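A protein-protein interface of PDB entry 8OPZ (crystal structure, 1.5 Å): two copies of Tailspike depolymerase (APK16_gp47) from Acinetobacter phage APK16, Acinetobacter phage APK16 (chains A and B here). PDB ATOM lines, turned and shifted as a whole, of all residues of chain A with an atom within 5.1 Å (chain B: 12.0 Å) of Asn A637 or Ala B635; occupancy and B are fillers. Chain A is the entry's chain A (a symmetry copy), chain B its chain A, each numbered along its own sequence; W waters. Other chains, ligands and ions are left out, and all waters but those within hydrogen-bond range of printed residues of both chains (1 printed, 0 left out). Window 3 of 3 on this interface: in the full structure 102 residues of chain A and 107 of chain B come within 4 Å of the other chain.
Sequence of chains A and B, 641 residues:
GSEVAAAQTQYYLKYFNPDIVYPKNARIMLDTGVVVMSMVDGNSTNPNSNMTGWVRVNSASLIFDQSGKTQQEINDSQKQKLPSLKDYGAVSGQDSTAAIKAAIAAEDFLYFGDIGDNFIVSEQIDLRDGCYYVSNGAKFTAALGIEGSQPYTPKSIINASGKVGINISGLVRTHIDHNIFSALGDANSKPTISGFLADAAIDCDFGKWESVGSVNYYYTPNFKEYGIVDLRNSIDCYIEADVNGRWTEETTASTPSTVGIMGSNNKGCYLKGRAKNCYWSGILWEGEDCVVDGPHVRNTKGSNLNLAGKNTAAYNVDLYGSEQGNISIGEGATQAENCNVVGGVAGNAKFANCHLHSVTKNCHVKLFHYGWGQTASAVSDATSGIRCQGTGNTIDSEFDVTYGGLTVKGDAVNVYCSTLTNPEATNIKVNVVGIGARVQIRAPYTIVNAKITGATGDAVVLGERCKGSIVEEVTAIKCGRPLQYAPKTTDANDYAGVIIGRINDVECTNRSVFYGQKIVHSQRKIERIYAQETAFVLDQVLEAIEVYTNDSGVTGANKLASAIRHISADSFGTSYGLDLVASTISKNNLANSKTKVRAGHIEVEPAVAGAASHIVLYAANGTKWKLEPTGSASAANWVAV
O of Ser B634 sits at hydrogen-bond distance from N of Trp A638 (2.9 Å).
The backbone NH of Ala B636 is in hydrogen-bond range of the backbone carbonyl oxygen of Ala A636.
NZ of Lys B626 is in salt-bridge range of OE2 of Glu B628, 3.1 Å away.
OG1 of Thr B630 lies within hydrogen-bond range of N of Ser B632.
The side-chain hydroxyl of Ser B634 sits at hydrogen-bond distance from the side-chain hydroxyl of Thr B630 (3.0 Å).
O of Ser B632 is in hydrogen-bond range of OG of Ser B634 (3.3 Å).
O of Ala B635 sits at hydrogen-bond distance from ND2 of Asn B637 (3.3 Å).
The backbone carbonyl oxygen of Ala A635 is in hydrogen-bond range of the side-chain amide nitrogen of Asn A637 (3.3 Å).
Leu B627 touches Leu A627 (CD1 to CD1, 3.7 Å).
Leu A627 touches Ala B636 (CD2 to CB, 3.8 Å).
O of Ala A636 touches CA of Ala B635, 3.6 Å away.
Asn A637 touches Ser B634.
Asn A637 touches Ala B635.
Trp A638 touches Leu B627.
Pro B629 touches Trp A638.
O of Ser B632 touches CB of Trp A638, at 3.6 Å.
O of Ala B635 touches CD1 of Trp A638, 3.9 Å away.
Ala B636 touches Trp A638 (CA to NE1, 3.6 Å).
Asn A637 touches two residues of chain B.
Of chain A, only Ala A636, Asn A637 and Trp A638 come within 4 Å of Ala B635.
No residue of chain B comes within 4 Å of Ala A635.
Ala A636 touches just these residues of chain B: Ala B635 (3.6 Å) and Ala B636 (2.7 Å).
Of chain B, only Leu B627 (3.7 Å), Glu B628 (3.4 Å), Pro B629 (3.6 Å), Ser B632 (3.6 Å), Ala B633 (3.2 Å), Ser B634 (2.9 Å), Ala B635 (3.9 Å) and Ala B636 (3.6 Å) come within 4 Å of Trp A638.
Of the printed residues of chain A, Glu B628 touches Trp A638.
Of the printed residues of chain A, Ser B634 touches Asn A637 (3.4 Å) and Trp A638 (2.9 Å).
Of the printed residues of chain A, Ser B632 touches Trp A638 (3.6 Å).
Ile B615 touches none of the printed residues of chain A.
The nearest residue of chain B that does not touch Asn A637 is Ala B636 (4.1 Å).
The nearest printed residue of chain A that does not touch Ala B633 is Asn A637 (5.0 Å).
Hydrophobic or aromatic side chains of chain A that line the printed part of chain B: Leu A627 and Trp A638.
Hydrophobic or aromatic side chains of chain B within 4 Å of the printed part of chain A: Leu B627, Pro B629, Ala B633 and Ala B636.
Along chain B the printed residues that touch a printed residue of chain A span positions 627 to 636.
Among the printed residues, 14 pairs touch across the chains.
Among the printed residues, no Asp or Glu carboxylate lies within 4 Å of a Lys or Arg side-chain nitrogen of the other chain.
Leu B627 touches its own counterpart, Leu A627.
Ala A636 touches Ala B635, but with the chains exchanged Ala A635 does not touch Ala B636 (6.2 Å).
Asn A637 touches Ala B635, but with the chains exchanged Ala A635 does not touch Asn B637 (8.2 Å).
Trp A638 touches Ala B636, but with the chains exchanged Ala A636 does not touch Trp B638 (7.6 Å).
Positions printed for both chains: 626, 627, 635, 636, 637, 638 and 639.
Of the 14 pairs that touch across the chains among the printed residues, 2 have their exchanged pair printed and touching as well.
Water W1 lies within hydrogen-bond range of the backbone carbonyl oxygen of Ala B636 and the backbone carbonyl oxygen of Ala A636.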
ATOM      1  N   LYS A 626       7.634   5.628  33.141  1.00  0.00           N
ATOM      2  CA  LYS A 626       7.448   7.066  33.279  1.00  0.00           C
ATOM      3  C   LYS A 626       8.505   7.776  32.469  1.00  0.00           C
ATOM      4  O   LYS A 626       9.681   7.346  32.521  1.00  0.00           O
ATOM      5  CB  LYS A 626       7.426   7.658  34.703  1.00  0.00           C
ATOM      6  CG  LYS A 626       8.395   7.136  35.774  1.00  0.00           C
ATOM      7  CD  LYS A 626       9.174   8.150  36.649  1.00  0.00           C
ATOM      8  CE  LYS A 626       8.837   8.175  38.135  1.00  0.00           C
ATOM      9  NZ  LYS A 626      10.007   8.610  38.960  1.00  0.00           N
ATOM     10  N   LEU A 627       8.032   8.825  31.757  1.00  0.00           N
ATOM     11  CA  LEU A 627       8.828   9.962  31.300  1.00  0.00           C
ATOM     12  C   LEU A 627       8.694  11.115  32.291  1.00  0.00           C
ATOM     13  O   LEU A 627       7.595  11.635  32.463  1.00  0.00           O
ATOM     14  CB  LEU A 627       8.422  10.428  29.891  1.00  0.00           C
ATOM     15  CG  LEU A 627       8.597   9.425  28.742  1.00  0.00           C
ATOM     16  CD1 LEU A 627       7.854   9.838  27.471  1.00  0.00           C
ATOM     17  CD2 LEU A 627      10.060   9.142  28.370  1.00  0.00           C
ATOM     18  N   ALA A 635      18.345  13.604  26.682  1.00  0.00           N
ATOM     19  CA  ALA A 635      17.547  12.518  26.131  1.00  0.00           C
ATOM     20  C   ALA A 635      16.538  12.044  27.181  1.00  0.00           C
ATOM     21  O   ALA A 635      16.883  11.944  28.371  1.00  0.00           O
ATOM     22  CB  ALA A 635      18.446  11.404  25.630  1.00  0.00           C
ATOM     23  N   ALA A 636      15.282  11.849  26.724  1.00  0.00           N
ATOM     24  CA  ALA A 636      14.247  11.237  27.546  1.00  0.00           C
ATOM     25  C   ALA A 636      14.371   9.732  27.428  1.00  0.00           C
ATOM     26  O   ALA A 636      14.510   9.184  26.327  1.00  0.00           O
ATOM     27  CB  ALA A 636      12.847  11.713  27.233  1.00  0.00           C
ATOM     28  N   ASN A 637      14.402   9.121  28.604  1.00  0.00           N
ATOM     29  CA  ASN A 637      14.433   7.678  28.791  1.00  0.00           C
ATOM     30  C   ASN A 637      13.211   7.267  29.594  1.00  0.00           C
ATOM     31  O   ASN A 637      12.846   7.931  30.561  1.00  0.00           O
ATOM     32  CB  ASN A 637      15.614   7.213  29.650  1.00  0.00           C
ATOM     33  CG  ASN A 637      16.897   7.869  29.196  1.00  0.00           C
ATOM     34  OD1 ASN A 637      17.467   7.439  28.205  1.00  0.00           O
ATOM     35  ND2 ASN A 637      17.268   8.984  29.810  1.00  0.00           N
ATOM     36  N   TRP A 638      12.756   6.051  29.261  1.00  0.00           N
ATOM     37  CA  TRP A 638      11.803   5.266  30.026  1.00  0.00           C
ATOM     38  C   TRP A 638      12.424   4.812  31.354  1.00  0.00           C
ATOM     39  O   TRP A 638      13.505   4.230  31.377  1.00  0.00           O
ATOM     40  CB  TRP A 638      11.275   4.114  29.168  1.00  0.00           C
ATOM     41  CG  TRP A 638      10.729   4.484  27.818  1.00  0.00           C
ATOM     42  CD1 TRP A 638      11.272   4.175  26.603  1.00  0.00           C
ATOM     43  CD2 TRP A 638       9.477   5.149  27.545  1.00  0.00           C
ATOM     44  NE1 TRP A 638      10.452   4.606  25.591  1.00  0.00           N
ATOM     45  CE2 TRP A 638       9.350   5.225  26.128  1.00  0.00           C
ATOM     46  CE3 TRP A 638       8.470   5.700  28.366  1.00  0.00           C
ATOM     47  CZ2 TRP A 638       8.247   5.862  25.520  1.00  0.00           C
ATOM     48  CZ3 TRP A 638       7.346   6.249  27.764  1.00  0.00           C
ATOM     49  CH2 TRP A 638       7.231   6.313  26.354  1.00  0.00           C
ATOM     50  N   VAL A 639      11.779   5.228  32.450  1.00  0.00           N
ATOM     51  CA  VAL A 639      12.128   4.935  33.843  1.00  0.00           C
ATOM     52  C   VAL A 639      11.034   4.047  34.438  1.00  0.00           C
ATOM     53  O   VAL A 639       9.853   4.395  34.384  1.00  0.00           O
ATOM     54  CB  VAL A 639      12.472   6.170  34.722  1.00  0.00           C
ATOM     55  CG1 VAL A 639      12.732   5.812  36.191  1.00  0.00           C
ATOM     56  CG2 VAL A 639      13.637   7.019  34.207  1.00  0.00           C
ATOM     57  N   ILE B 615       1.245   8.196  24.060  1.00  0.00           N
ATOM     58  CA  ILE B 615       0.942   9.619  23.841  1.00  0.00           C
ATOM     59  C   ILE B 615       1.224   9.949  22.366  1.00  0.00           C
ATOM     60  O   ILE B 615       2.349   9.676  21.872  1.00  0.00           O
ATOM     61  CB  ILE B 615       1.553  10.664  24.836  1.00  0.00           C
ATOM     62  CG1 ILE B 615       0.834  11.997  24.593  1.00  0.00           C
ATOM     63  CG2 ILE B 615       3.085  10.773  24.888  1.00  0.00           C
ATOM     64  CD1 ILE B 615       1.100  13.206  25.453  1.00  0.00           C
ATOM     65  N   LYS B 626       4.173   9.098  18.200  1.00  0.00           N
ATOM     66  CA  LYS B 626       3.849   8.471  19.474  1.00  0.00           C
ATOM     67  C   LYS B 626       5.130   8.198  20.224  1.00  0.00           C
ATOM     68  O   LYS B 626       6.101   7.728  19.589  1.00  0.00           O
ATOM     69  CB  LYS B 626       2.998   7.184  19.450  1.00  0.00           C
ATOM     70  CG  LYS B 626       3.237   6.118  18.371  1.00  0.00           C
ATOM     71  CD  LYS B 626       3.327   4.628  18.786  1.00  0.00           C
ATOM     72  CE  LYS B 626       2.218   3.708  18.288  1.00  0.00           C
ATOM     73  NZ  LYS B 626       2.699   2.301  18.127  1.00  0.00           N
ATOM     74  N   LEU B 627       5.067   8.512  21.539  1.00  0.00           N
ATOM     75  CA  LEU B 627       5.907   7.933  22.586  1.00  0.00           C
ATOM     76  C   LEU B 627       5.168   6.779  23.258  1.00  0.00           C
ATOM     77  O   LEU B 627       4.129   7.007  23.871  1.00  0.00           O
ATOM     78  CB  LEU B 627       6.326   8.974  23.638  1.00  0.00           C
ATOM     79  CG  LEU B 627       7.177  10.157  23.154  1.00  0.00           C
ATOM     80  CD1 LEU B 627       7.244  11.299  24.170  1.00  0.00           C
ATOM     81  CD2 LEU B 627       8.614   9.781  22.762  1.00  0.00           C
ATOM     82  N   GLU B 628       5.771   5.578  23.172  1.00  0.00           N
ATOM     83  CA  GLU B 628       5.255   4.250  23.540  1.00  0.00           C
ATOM     84  C   GLU B 628       6.384   3.391  24.138  1.00  0.00           C
ATOM     85  O   GLU B 628       7.389   3.123  23.433  1.00  0.00           O
ATOM     86  CB  GLU B 628       4.575   3.560  22.337  1.00  0.00           C
ATOM     87  CG  GLU B 628       3.959   2.185  22.618  1.00  0.00           C
ATOM     88  CD  GLU B 628       3.213   1.436  21.509  1.00  0.00           C
ATOM     89  OE1 GLU B 628       3.771   0.424  21.009  1.00  0.00           O
ATOM     90  OE2 GLU B 628       2.087   1.889  21.146  1.00  0.00           O
ATOM     91  N   PRO B 629       6.256   2.899  25.411  1.00  0.00           N
ATOM     92  CA  PRO B 629       7.365   2.160  26.061  1.00  0.00           C
ATOM     93  C   PRO B 629       7.728   0.822  25.423  1.00  0.00           C
ATOM     94  O   PRO B 629       6.855   0.139  24.892  1.00  0.00           O
ATOM     95  CB  PRO B 629       6.798   1.895  27.471  1.00  0.00           C
ATOM     96  CG  PRO B 629       5.789   2.981  27.654  1.00  0.00           C
ATOM     97  CD  PRO B 629       5.086   2.998  26.320  1.00  0.00           C
ATOM     98  N   THR B 630       9.002   0.458  25.594  1.00  0.00           N
ATOM     99  CA  THR B 630       9.653  -0.627  24.862  1.00  0.00           C
ATOM    100  C   THR B 630       9.547  -1.925  25.671  1.00  0.00           C
ATOM    101  O   THR B 630       9.783  -3.006  25.139  1.00  0.00           O
ATOM    102  CB  THR B 630      11.107  -0.286  24.445  1.00  0.00           C
ATOM    103  OG1 THR B 630      11.877  -0.158  25.644  1.00  0.00           O
ATOM    104  CG2 THR B 630      11.252   0.954  23.564  1.00  0.00           C
ATOM    105  N   GLY B 631       9.249  -1.806  26.973  1.00  0.00           N
ATOM    106  CA  GLY B 631       9.480  -2.824  27.977  1.00  0.00           C
ATOM    107  C   GLY B 631      10.926  -2.860  28.462  1.00  0.00           C
ATOM    108  O   GLY B 631      11.297  -3.857  29.065  1.00  0.00           O
ATOM    109  N   SER B 632      11.705  -1.781  28.200  1.00  0.00           N
ATOM    110  CA  SER B 632      12.996  -1.533  28.838  1.00  0.00           C
ATOM    111  C   SER B 632      13.222  -0.050  29.151  1.00  0.00           C
ATOM    112  O   SER B 632      12.561   0.837  28.585  1.00  0.00           O
ATOM    113  CB  SER B 632      14.176  -2.217  28.143  1.00  0.00           C
ATOM    114  OG  SER B 632      14.173  -2.009  26.739  1.00  0.00           O
ATOM    115  N   ALA B 633      14.184   0.151  30.075  1.00  0.00           N
ATOM    116  CA  ALA B 633      14.704   1.362  30.685  1.00  0.00           C
ATOM    117  C   ALA B 633      15.681   2.072  29.740  1.00  0.00           C
ATOM    118  O   ALA B 633      16.821   2.369  30.107  1.00  0.00           O
ATOM    119  CB  ALA B 633      15.273   0.952  32.043  1.00  0.00           C
ATOM    120  N   SER B 634      15.153   2.443  28.556  1.00  0.00           N
ATOM    121  CA  SER B 634      15.852   2.796  27.316  1.00  0.00           C
ATOM    122  C   SER B 634      15.395   4.159  26.810  1.00  0.00           C
ATOM    123  O   SER B 634      14.368   4.653  27.266  1.00  0.00           O
ATOM    124  CB  SER B 634      15.604   1.718  26.275  1.00  0.00           C
ATOM    125  OG  SER B 634      14.222   1.683  25.904  1.00  0.00           O
ATOM    126  N   ALA B 635      16.121   4.715  25.822  1.00  0.00           N
ATOM    127  CA  ALA B 635      15.838   6.010  25.219  1.00  0.00           C
ATOM    128  C   ALA B 635      14.449   5.980  24.576  1.00  0.00           C
ATOM    129  O   ALA B 635      14.077   4.971  23.952  1.00  0.00           O
ATOM    130  CB  ALA B 635      16.934   6.386  24.240  1.00  0.00           C
ATOM    131  N   ALA B 636      13.677   7.060  24.826  1.00  0.00           N
ATOM    132  CA  ALA B 636      12.401   7.270  24.153  1.00  0.00           C
ATOM    133  C   ALA B 636      12.668   7.944  22.824  1.00  0.00           C
ATOM    134  O   ALA B 636      13.433   8.913  22.738  1.00  0.00           O
ATOM    135  CB  ALA B 636      11.387   8.029  24.977  1.00  0.00           C
ATOM    136  N   ASN B 637      12.078   7.333  21.805  1.00  0.00           N
ATOM    137  CA  ASN B 637      12.092   7.806  20.430  1.00  0.00           C
ATOM    138  C   ASN B 637      10.660   8.042  19.982  1.00  0.00           C
ATOM    139  O   ASN B 637       9.776   7.239  20.269  1.00  0.00           O
ATOM    140  CB  ASN B 637      12.621   6.759  19.443  1.00  0.00           C
ATOM    141  CG  ASN B 637      13.893   6.130  19.963  1.00  0.00           C
ATOM    142  OD1 ASN B 637      14.946   6.741  19.855  1.00  0.00           O
ATOM    143  ND2 ASN B 637      13.785   5.002  20.650  1.00  0.00           N
ATOM    144  N   TRP B 638      10.548   9.053  19.110  1.00  0.00           N
ATOM    145  CA  TRP B 638       9.384   9.335  18.288  1.00  0.00           C
ATOM    146  C   TRP B 638       9.187   8.236  17.238  1.00  0.00           C
ATOM    147  O   TRP B 638      10.106   7.902  16.494  1.00  0.00           O
ATOM    148  CB  TRP B 638       9.500  10.742  17.693  1.00  0.00           C
ATOM    149  CG  TRP B 638       9.778  11.854  18.664  1.00  0.00           C
ATOM    150  CD1 TRP B 638      10.924  12.591  18.758  1.00  0.00           C
ATOM    151  CD2 TRP B 638       8.850  12.426  19.612  1.00  0.00           C
ATOM    152  NE1 TRP B 638      10.782  13.576  19.703  1.00  0.00           N
ATOM    153  CE2 TRP B 638       9.531  13.495  20.262  1.00  0.00           C
ATOM    154  CE3 TRP B 638       7.524  12.116  19.981  1.00  0.00           C
ATOM    155  CZ2 TRP B 638       8.916  14.243  21.289  1.00  0.00           C
ATOM    156  CZ3 TRP B 638       6.894  12.910  20.929  1.00  0.00           C
ATOM    157  CH2 TRP B 638       7.581  13.973  21.564  1.00  0.00           C
ATOM    158  N   VAL B 639       8.015   7.593  17.305  1.00  0.00           N
ATOM    159  CA  VAL B 639       7.545   6.519  16.426  1.00  0.00           C
ATOM    160  C   VAL B 639       6.366   7.045  15.607  1.00  0.00           C
ATOM    161  O   VAL B 639       5.397   7.556  16.171  1.00  0.00           O
ATOM    162  CB  VAL B 639       7.260   5.159  17.123  1.00  0.00           C
ATOM    163  CG1 VAL B 639       6.679   4.103  16.172  1.00  0.00           C
ATOM    164  CG2 VAL B 639       8.456   4.553  17.862  1.00  0.00           C
HETATM  165  O   HOH W   1      16.065   9.683  23.855  1.00  0.00           O
